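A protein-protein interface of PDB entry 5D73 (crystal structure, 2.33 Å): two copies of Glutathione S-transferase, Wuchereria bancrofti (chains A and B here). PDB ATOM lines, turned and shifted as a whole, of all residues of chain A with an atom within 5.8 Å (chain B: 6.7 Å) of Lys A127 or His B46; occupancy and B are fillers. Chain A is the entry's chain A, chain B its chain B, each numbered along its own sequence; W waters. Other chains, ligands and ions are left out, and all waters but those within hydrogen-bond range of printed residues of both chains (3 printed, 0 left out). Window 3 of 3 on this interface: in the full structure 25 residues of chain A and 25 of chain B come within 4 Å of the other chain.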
ATOM      1  N   MET A  89      -6.455 -18.464  14.585  1.00  0.00           N
ATOM      2  CA  MET A  89      -7.897 -18.692  14.524  1.00  0.00           C
ATOM      3  C   MET A  89      -8.599 -17.559  13.736  1.00  0.00           C
ATOM      4  O   MET A  89      -9.379 -17.816  12.834  1.00  0.00           O
ATOM      5  CB  MET A  89      -8.356 -18.856  15.977  1.00  0.00           C
ATOM      6  CG  MET A  89      -9.776 -19.198  16.249  1.00  0.00           C
ATOM      7  SD  MET A  89      -9.968 -19.618  17.992  1.00  0.00           S
ATOM      8  CE  MET A  89     -10.021 -17.976  18.711  1.00  0.00           C
ATOM      9  N   PHE A  90      -8.227 -16.316  13.989  1.00  0.00           N
ATOM     10  CA  PHE A  90      -8.828 -15.176  13.289  1.00  0.00           C
ATOM     11  C   PHE A  90      -8.391 -15.214  11.830  1.00  0.00           C
ATOM     12  O   PHE A  90      -9.227 -15.020  10.924  1.00  0.00           O
ATOM     13  CB  PHE A  90      -8.374 -13.836  13.918  1.00  0.00           C
ATOM     14  CG  PHE A  90      -9.396 -12.704  13.851  1.00  0.00           C
ATOM     15  CD1 PHE A  90      -9.608 -11.883  14.966  1.00  0.00           C
ATOM     16  CD2 PHE A  90     -10.134 -12.454  12.705  1.00  0.00           C
ATOM     17  CE1 PHE A  90     -10.543 -10.835  14.930  1.00  0.00           C
ATOM     18  CE2 PHE A  90     -11.079 -11.427  12.675  1.00  0.00           C
ATOM     19  CZ  PHE A  90     -11.276 -10.603  13.784  1.00  0.00           C
ATOM     20  N   PRO A 122     -22.889  -9.930   5.345  1.00  0.00           N
ATOM     21  CA  PRO A 122     -23.151  -9.391   6.682  1.00  0.00           C
ATOM     22  C   PRO A 122     -23.042 -10.442   7.782  1.00  0.00           C
ATOM     23  O   PRO A 122     -22.567 -10.146   8.884  1.00  0.00           O
ATOM     24  CB  PRO A 122     -24.577  -8.828   6.572  1.00  0.00           C
ATOM     25  CG  PRO A 122     -24.787  -8.539   5.110  1.00  0.00           C
ATOM     26  CD  PRO A 122     -23.994  -9.632   4.408  1.00  0.00           C
ATOM     27  N   VAL A 123     -23.439 -11.672   7.479  1.00  0.00           N
ATOM     28  CA  VAL A 123     -23.360 -12.739   8.478  1.00  0.00           C
ATOM     29  C   VAL A 123     -21.909 -13.033   8.860  1.00  0.00           C
ATOM     30  O   VAL A 123     -21.594 -13.270  10.053  1.00  0.00           O
ATOM     31  CB  VAL A 123     -24.194 -13.984   8.057  1.00  0.00           C
ATOM     32  CG1 VAL A 123     -24.099 -15.105   9.072  1.00  0.00           C
ATOM     33  CG2 VAL A 123     -25.684 -13.597   7.945  1.00  0.00           C
ATOM     34  N   GLU A 124     -21.028 -12.963   7.874  1.00  0.00           N
ATOM     35  CA  GLU A 124     -19.647 -13.301   8.087  1.00  0.00           C
ATOM     36  C   GLU A 124     -18.853 -12.173   8.750  1.00  0.00           C
ATOM     37  O   GLU A 124     -17.896 -12.444   9.520  1.00  0.00           O
ATOM     38  CB  GLU A 124     -18.959 -13.741   6.787  1.00  0.00           C
ATOM     39  CG  GLU A 124     -19.447 -15.046   6.212  1.00  0.00           C
ATOM     40  CD  GLU A 124     -19.486 -16.184   7.212  1.00  0.00           C
ATOM     41  OE1 GLU A 124     -18.437 -16.599   7.775  1.00  0.00           O
ATOM     42  OE2 GLU A 124     -20.611 -16.670   7.448  1.00  0.00           O
ATOM     43  N   LEU A 125     -19.248 -10.925   8.449  1.00  0.00           N
ATOM     44  CA  LEU A 125     -18.627  -9.753   9.065  1.00  0.00           C
ATOM     45  C   LEU A 125     -19.000  -9.596  10.553  1.00  0.00           C
ATOM     46  O   LEU A 125     -18.153  -9.236  11.367  1.00  0.00           O
ATOM     47  CB  LEU A 125     -18.908  -8.486   8.241  1.00  0.00           C
ATOM     48  CG  LEU A 125     -18.292  -8.434   6.844  1.00  0.00           C
ATOM     49  CD1 LEU A 125     -18.759  -7.185   6.126  1.00  0.00           C
ATOM     50  CD2 LEU A 125     -16.778  -8.484   6.879  1.00  0.00           C
ATOM     51  N   ALA A 126     -20.231  -9.940  10.911  1.00  0.00           N
ATOM     52  CA  ALA A 126     -20.662  -9.991  12.337  1.00  0.00           C
ATOM     53  C   ALA A 126     -19.746 -10.844  13.208  1.00  0.00           C
ATOM     54  O   ALA A 126     -19.502 -10.504  14.353  1.00  0.00           O
ATOM     55  CB  ALA A 126     -22.104 -10.496  12.475  1.00  0.00           C
ATOM     56  N   LYS A 127     -19.260 -11.948  12.657  1.00  0.00           N
ATOM     57  CA  LYS A 127     -18.311 -12.828  13.357  1.00  0.00           C
ATOM     58  C   LYS A 127     -16.969 -12.184  13.654  1.00  0.00           C
ATOM     59  O   LYS A 127     -16.454 -12.343  14.746  1.00  0.00           O
ATOM     60  CB  LYS A 127     -18.082 -14.093  12.552  1.00  0.00           C
ATOM     61  CG  LYS A 127     -19.282 -15.021  12.559  1.00  0.00           C
ATOM     62  CD  LYS A 127     -19.285 -15.952  11.356  1.00  0.00           C
ATOM     63  CE  LYS A 127     -20.574 -16.768  11.352  1.00  0.00           C
ATOM     64  NZ  LYS A 127     -20.522 -17.821  10.300  1.00  0.00           N
ATOM     65  N   PHE A 128     -16.427 -11.451  12.684  1.00  0.00           N
ATOM     66  CA  PHE A 128     -15.185 -10.668  12.868  1.00  0.00           C
ATOM     67  C   PHE A 128     -15.345  -9.487  13.817  1.00  0.00           C
ATOM     68  O   PHE A 128     -14.465  -9.225  14.659  1.00  0.00           O
ATOM     69  CB  PHE A 128     -14.698 -10.125  11.518  1.00  0.00           C
ATOM     70  CG  PHE A 128     -14.364 -11.191  10.480  1.00  0.00           C
ATOM     71  CD1 PHE A 128     -14.164 -12.539  10.819  1.00  0.00           C
ATOM     72  CD2 PHE A 128     -14.173 -10.823   9.174  1.00  0.00           C
ATOM     73  CE1 PHE A 128     -13.820 -13.480   9.851  1.00  0.00           C
ATOM     74  CE2 PHE A 128     -13.809 -11.762   8.203  1.00  0.00           C
ATOM     75  CZ  PHE A 128     -13.642 -13.078   8.542  1.00  0.00           C
ATOM     76  N   GLU A 129     -16.443  -8.746  13.649  1.00  0.00           N
ATOM     77  CA  GLU A 129     -16.808  -7.628  14.540  1.00  0.00           C
ATOM     78  C   GLU A 129     -16.833  -8.034  15.999  1.00  0.00           C
ATOM     79  O   GLU A 129     -16.223  -7.377  16.855  1.00  0.00           O
ATOM     80  CB  GLU A 129     -18.186  -7.052  14.169  1.00  0.00           C
ATOM     81  CG  GLU A 129     -18.662  -5.885  15.043  1.00  0.00           C
ATOM     82  CD  GLU A 129     -18.114  -4.496  14.622  1.00  0.00           C
ATOM     83  OE1 GLU A 129     -17.338  -4.370  13.659  1.00  0.00           O
ATOM     84  OE2 GLU A 129     -18.544  -3.504  15.249  1.00  0.00           O
ATOM     85  N   LYS A 130     -17.557  -9.095  16.282  1.00  0.00           N
ATOM     86  CA  LYS A 130     -17.619  -9.645  17.641  1.00  0.00           C
ATOM     87  C   LYS A 130     -16.238 -10.073  18.198  1.00  0.00           C
ATOM     88  O   LYS A 130     -15.888  -9.802  19.329  1.00  0.00           O
ATOM     89  CB  LYS A 130     -18.603 -10.823  17.650  1.00  0.00           C
ATOM     90  CG  LYS A 130     -18.826 -11.435  19.027  1.00  0.00           C
ATOM     91  CD  LYS A 130     -19.865 -12.555  18.919  1.00  0.00           C
ATOM     92  CE  LYS A 130     -20.136 -13.243  20.246  1.00  0.00           C
ATOM     93  NZ  LYS A 130     -21.418 -13.992  20.165  1.00  0.00           N
ATOM     94  N   LEU A 131     -15.461 -10.753  17.380  1.00  0.00           N
ATOM     95  CA  LEU A 131     -14.174 -11.255  17.811  1.00  0.00           C
ATOM     96  C   LEU A 131     -13.186 -10.094  18.057  1.00  0.00           C
ATOM     97  O   LEU A 131     -12.526 -10.042  19.099  1.00  0.00           O
ATOM     98  CB  LEU A 131     -13.659 -12.262  16.778  1.00  0.00           C
ATOM     99  CG  LEU A 131     -12.611 -13.283  17.203  1.00  0.00           C
ATOM    100  CD1 LEU A 131     -12.961 -13.996  18.495  1.00  0.00           C
ATOM    101  CD2 LEU A 131     -12.376 -14.305  16.099  1.00  0.00           C
ATOM    102  N   LEU A 132     -13.162  -9.130  17.139  1.00  0.00           N
ATOM    103  CA  LEU A 132     -12.355  -7.920  17.299  1.00  0.00           C
ATOM    104  C   LEU A 132     -12.658  -7.179  18.623  1.00  0.00           C
ATOM    105  O   LEU A 132     -11.751  -6.676  19.259  1.00  0.00           O
ATOM    106  CB  LEU A 132     -12.528  -6.994  16.068  1.00  0.00           C
ATOM    107  CG  LEU A 132     -11.823  -5.623  16.105  1.00  0.00           C
ATOM    108  CD1 LEU A 132     -10.325  -5.801  16.356  1.00  0.00           C
ATOM    109  CD2 LEU A 132     -12.086  -4.755  14.872  1.00  0.00           C
ATOM    110  N   LYS B  42     -24.882 -23.858  17.466  1.00  0.00           N
ATOM    111  CA  LYS B  42     -24.163 -23.118  16.415  1.00  0.00           C
ATOM    112  C   LYS B  42     -23.593 -21.743  16.834  1.00  0.00           C
ATOM    113  O   LYS B  42     -22.414 -21.452  16.609  1.00  0.00           O
ATOM    114  CB  LYS B  42     -25.076 -22.953  15.189  1.00  0.00           C
ATOM    115  CG  LYS B  42     -24.419 -22.355  13.939  1.00  0.00           C
ATOM    116  CD  LYS B  42     -25.411 -22.256  12.751  1.00  0.00           C
ATOM    117  CE  LYS B  42     -24.940 -21.228  11.734  1.00  0.00           C
ATOM    118  NZ  LYS B  42     -23.611 -21.611  11.171  1.00  0.00           N
ATOM    119  N   SER B  43     -24.426 -20.927  17.466  1.00  0.00           N
ATOM    120  CA  SER B  43     -24.061 -19.570  17.878  1.00  0.00           C
ATOM    121  C   SER B  43     -23.033 -19.505  19.041  1.00  0.00           C
ATOM    122  O   SER B  43     -22.480 -18.466  19.299  1.00  0.00           O
ATOM    123  CB  SER B  43     -25.355 -18.802  18.233  1.00  0.00           C
ATOM    124  OG  SER B  43     -25.866 -19.254  19.492  1.00  0.00           O
ATOM    125  N   HIS B  44     -22.802 -20.619  19.726  1.00  0.00           N
ATOM    126  CA  HIS B  44     -21.833 -20.725  20.816  1.00  0.00           C
ATOM    127  C   HIS B  44     -20.351 -20.682  20.355  1.00  0.00           C
ATOM    128  O   HIS B  44     -19.465 -20.443  21.177  1.00  0.00           O
ATOM    129  CB  HIS B  44     -22.023 -22.042  21.610  1.00  0.00           C
ATOM    130  CG  HIS B  44     -23.396 -22.246  22.174  1.00  0.00           C
ATOM    131  ND1 HIS B  44     -23.690 -23.271  23.049  1.00  0.00           N
ATOM    132  CD2 HIS B  44     -24.554 -21.562  22.000  1.00  0.00           C
ATOM    133  CE1 HIS B  44     -24.970 -23.233  23.354  1.00  0.00           C
ATOM    134  NE2 HIS B  44     -25.509 -22.195  22.752  1.00  0.00           N
ATOM    135  N   PHE B  45     -20.093 -20.917  19.067  1.00  0.00           N
ATOM    136  CA  PHE B  45     -18.720 -20.985  18.530  1.00  0.00           C
ATOM    137  C   PHE B  45     -18.344 -19.727  17.746  1.00  0.00           C
ATOM    138  O   PHE B  45     -19.207 -19.087  17.215  1.00  0.00           O
ATOM    139  CB  PHE B  45     -18.563 -22.277  17.745  1.00  0.00           C
ATOM    140  CG  PHE B  45     -18.938 -23.455  18.564  1.00  0.00           C
ATOM    141  CD1 PHE B  45     -18.086 -23.931  19.508  1.00  0.00           C
ATOM    142  CD2 PHE B  45     -20.203 -24.004  18.477  1.00  0.00           C
ATOM    143  CE1 PHE B  45     -18.464 -24.955  20.339  1.00  0.00           C
ATOM    144  CE2 PHE B  45     -20.570 -25.075  19.269  1.00  0.00           C
ATOM    145  CZ  PHE B  45     -19.700 -25.537  20.205  1.00  0.00           C
ATOM    146  N   HIS B  46     -17.071 -19.346  17.725  1.00  0.00           N
ATOM    147  CA  HIS B  46     -16.698 -18.026  17.208  1.00  0.00           C
ATOM    148  C   HIS B  46     -17.152 -17.849  15.772  1.00  0.00           C
ATOM    149  O   HIS B  46     -17.509 -16.749  15.392  1.00  0.00           O
ATOM    150  CB  HIS B  46     -15.195 -17.745  17.267  1.00  0.00           C
ATOM    151  CG  HIS B  46     -14.634 -17.638  18.652  1.00  0.00           C
ATOM    152  ND1 HIS B  46     -15.201 -16.849  19.637  1.00  0.00           N
ATOM    153  CD2 HIS B  46     -13.522 -18.186  19.209  1.00  0.00           C
ATOM    154  CE1 HIS B  46     -14.467 -16.915  20.743  1.00  0.00           C
ATOM    155  NE2 HIS B  46     -13.443 -17.723  20.512  1.00  0.00           N
ATOM    156  N   PHE B  47     -17.102 -18.901  14.952  1.00  0.00           N
ATOM    157  CA  PHE B  47     -17.464 -18.760  13.519  1.00  0.00           C
ATOM    158  C   PHE B  47     -18.739 -19.520  13.128  1.00  0.00           C
ATOM    159  O   PHE B  47     -19.011 -19.715  11.922  1.00  0.00           O
ATOM    160  CB  PHE B  47     -16.265 -19.161  12.612  1.00  0.00           C
ATOM    161  CG  PHE B  47     -15.041 -18.291  12.801  1.00  0.00           C
ATOM    162  CD1 PHE B  47     -15.075 -16.952  12.496  1.00  0.00           C
ATOM    163  CD2 PHE B  47     -13.851 -18.824  13.282  1.00  0.00           C
ATOM    164  CE1 PHE B  47     -13.968 -16.150  12.669  1.00  0.00           C
ATOM    165  CE2 PHE B  47     -12.729 -18.044  13.439  1.00  0.00           C
ATOM    166  CZ  PHE B  47     -12.786 -16.695  13.133  1.00  0.00           C
ATOM    167  N   GLY B  48     -19.494 -19.947  14.137  1.00  0.00           N
ATOM    168  CA  GLY B  48     -20.624 -20.836  13.937  1.00  0.00           C
ATOM    169  C   GLY B  48     -20.357 -22.162  13.252  1.00  0.00           C
ATOM    170  O   GLY B  48     -21.221 -22.670  12.538  1.00  0.00           O
ATOM    171  N   GLN B  49     -19.174 -22.722  13.480  1.00  0.00           N
ATOM    172  CA  GLN B  49     -18.774 -24.010  12.883  1.00  0.00           C
ATOM    173  C   GLN B  49     -17.938 -24.856  13.841  1.00  0.00           C
ATOM    174  O   GLN B  49     -17.583 -24.411  14.938  1.00  0.00           O
ATOM    175  CB  GLN B  49     -17.988 -23.801  11.581  1.00  0.00           C
ATOM    176  CG  GLN B  49     -18.759 -23.092  10.496  1.00  0.00           C
ATOM    177  CD  GLN B  49     -18.197 -23.307   9.088  1.00  0.00           C
ATOM    178  OE1 GLN B  49     -18.922 -23.738   8.198  1.00  0.00           O
ATOM    179  NE2 GLN B  49     -16.938 -22.980   8.881  1.00  0.00           N
ATOM    180  N   GLN B  59     -11.723 -21.448  24.246  1.00  0.00           N
ATOM    181  CA  GLN B  59     -12.367 -21.968  23.033  1.00  0.00           C
ATOM    182  C   GLN B  59     -11.423 -21.867  21.831  1.00  0.00           C
ATOM    183  O   GLN B  59     -10.990 -20.780  21.479  1.00  0.00           O
ATOM    184  CB  GLN B  59     -13.645 -21.188  22.737  1.00  0.00           C
ATOM    185  CG  GLN B  59     -14.406 -21.716  21.533  1.00  0.00           C
ATOM    186  CD  GLN B  59     -15.503 -20.794  21.041  1.00  0.00           C
ATOM    187  OE1 GLN B  59     -15.795 -20.755  19.842  1.00  0.00           O
ATOM    188  NE2 GLN B  59     -16.135 -20.070  21.950  1.00  0.00           N
ATOM    189  N   ILE B  60     -11.125 -22.994  21.187  1.00  0.00           N
ATOM    190  CA  ILE B  60     -10.285 -22.973  19.975  1.00  0.00           C
ATOM    191  C   ILE B  60     -11.021 -23.627  18.813  1.00  0.00           C
ATOM    192  O   ILE B  60     -11.171 -24.891  18.755  1.00  0.00           O
ATOM    193  CB  ILE B  60      -8.894 -23.605  20.161  1.00  0.00           C
ATOM    194  CG1 ILE B  60      -8.164 -22.995  21.373  1.00  0.00           C
ATOM    195  CG2 ILE B  60      -8.053 -23.345  18.914  1.00  0.00           C
ATOM    196  CD1 ILE B  60      -6.895 -23.738  21.818  1.00  0.00           C
ATOM    197  N   VAL B  61     -11.481 -22.760  17.900  1.00  0.00           N
ATOM    198  CA  VAL B  61     -12.022 -23.226  16.641  1.00  0.00           C
ATOM    199  C   VAL B  61     -10.956 -23.142  15.543  1.00  0.00           C
ATOM    200  O   VAL B  61      -9.842 -22.692  15.804  1.00  0.00           O
ATOM    201  CB  VAL B  61     -13.355 -22.547  16.281  1.00  0.00           C
ATOM    202  CG1 VAL B  61     -14.409 -23.008  17.273  1.00  0.00           C
ATOM    203  CG2 VAL B  61     -13.256 -21.024  16.244  1.00  0.00           C
HETATM  204  O   HOH W   1     -23.143 -16.267  18.436  1.00  0.00           O
HETATM  205  O   HOH W   2     -17.433 -14.352  16.399  1.00  0.00           O
HETATM  206  O   HOH W   3     -22.700 -18.833  10.070  1.00  0.00           O
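SD of Met A89 sits at hydrogen-bond distance from N of Val B61 (3.5 Å). The backbone carbonyl oxygen of Phe B47 is in hydrogen-bond range of the side-chain amino group of Lys A127, 2.9 Å away.
OE2 of Glu A124 lies within salt-bridge range of NZ of Lys A127, at 3.1 Å. The side-chain amide nitrogen (NE2) of Gln B59 lies within hydrogen-bond range of the backbone carbonyl oxygen (O) of His B44 (3.4 Å). N of His B46 sits at hydrogen-bond distance from OE1 of Gln B59 (2.8 Å).
Among the printed residues, merely in contact across the chains: Met A89 with His B46, Met A89 with Phe B47, Met A89 with Gln B59, Met A89 with Ile B60, Lys A127 with His B46, Phe A128 with Phe B47, Leu A131 with His B46 and Leu A131 with Phe B47.
Of chain B, only His B46 and Phe B47 come within 4 Å of Lys A127. His B46 touches just these residues of chain A: Met A89, Lys A127 and Leu A131. Printed residues of chain A within 4 Å of Ile B60: Met A89. Of the printed residues of chain B, Leu A131 touches His B46 (3.8 Å) and Phe B47 (3.8 Å). Of the printed residues of chain B, Met A89 touches His B46, Phe B47, Gln B59, Ile B60 and Val B61. Of the printed residues of chain A, Val B61 touches Met A89. Of the printed residues of chain B, Phe A128 touches Phe B47. Ser B43 touches none of the printed residues of chain A. Phe A90 touches none of the printed residues of chain B.
Hydrophobic or aromatic side chains of chain A within 4 Å of the printed part of chain B: Met A89, Phe A128 and Leu A131. Hydrophobic or aromatic side chains of chain B within 4 Å of the printed part of chain A: His B46, Phe B47 and Val B61. Among the printed residues, 10 pairs touch across the chains. Among the printed residues, no Asp or Glu carboxylate lies within 4 Å of a Lys or Arg side-chain nitrogen of the other chain.
No position is printed for both chains. Of the 10 pairs that touch across the chains among the printed residues, none has its exchanged pair printed and touching as well.
Water W3 lies within hydrogen-bond range of the side-chain amino group (NZ) of Lys A127 (2.4 Å) and the side-chain amino group (NZ) of Lys B42 (3.1 Å). Water W1 bridges O of Ser B43 and NZ of Lys A130. Water W2 lies within hydrogen-bond range of O of His B46 and O of Lys A127.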
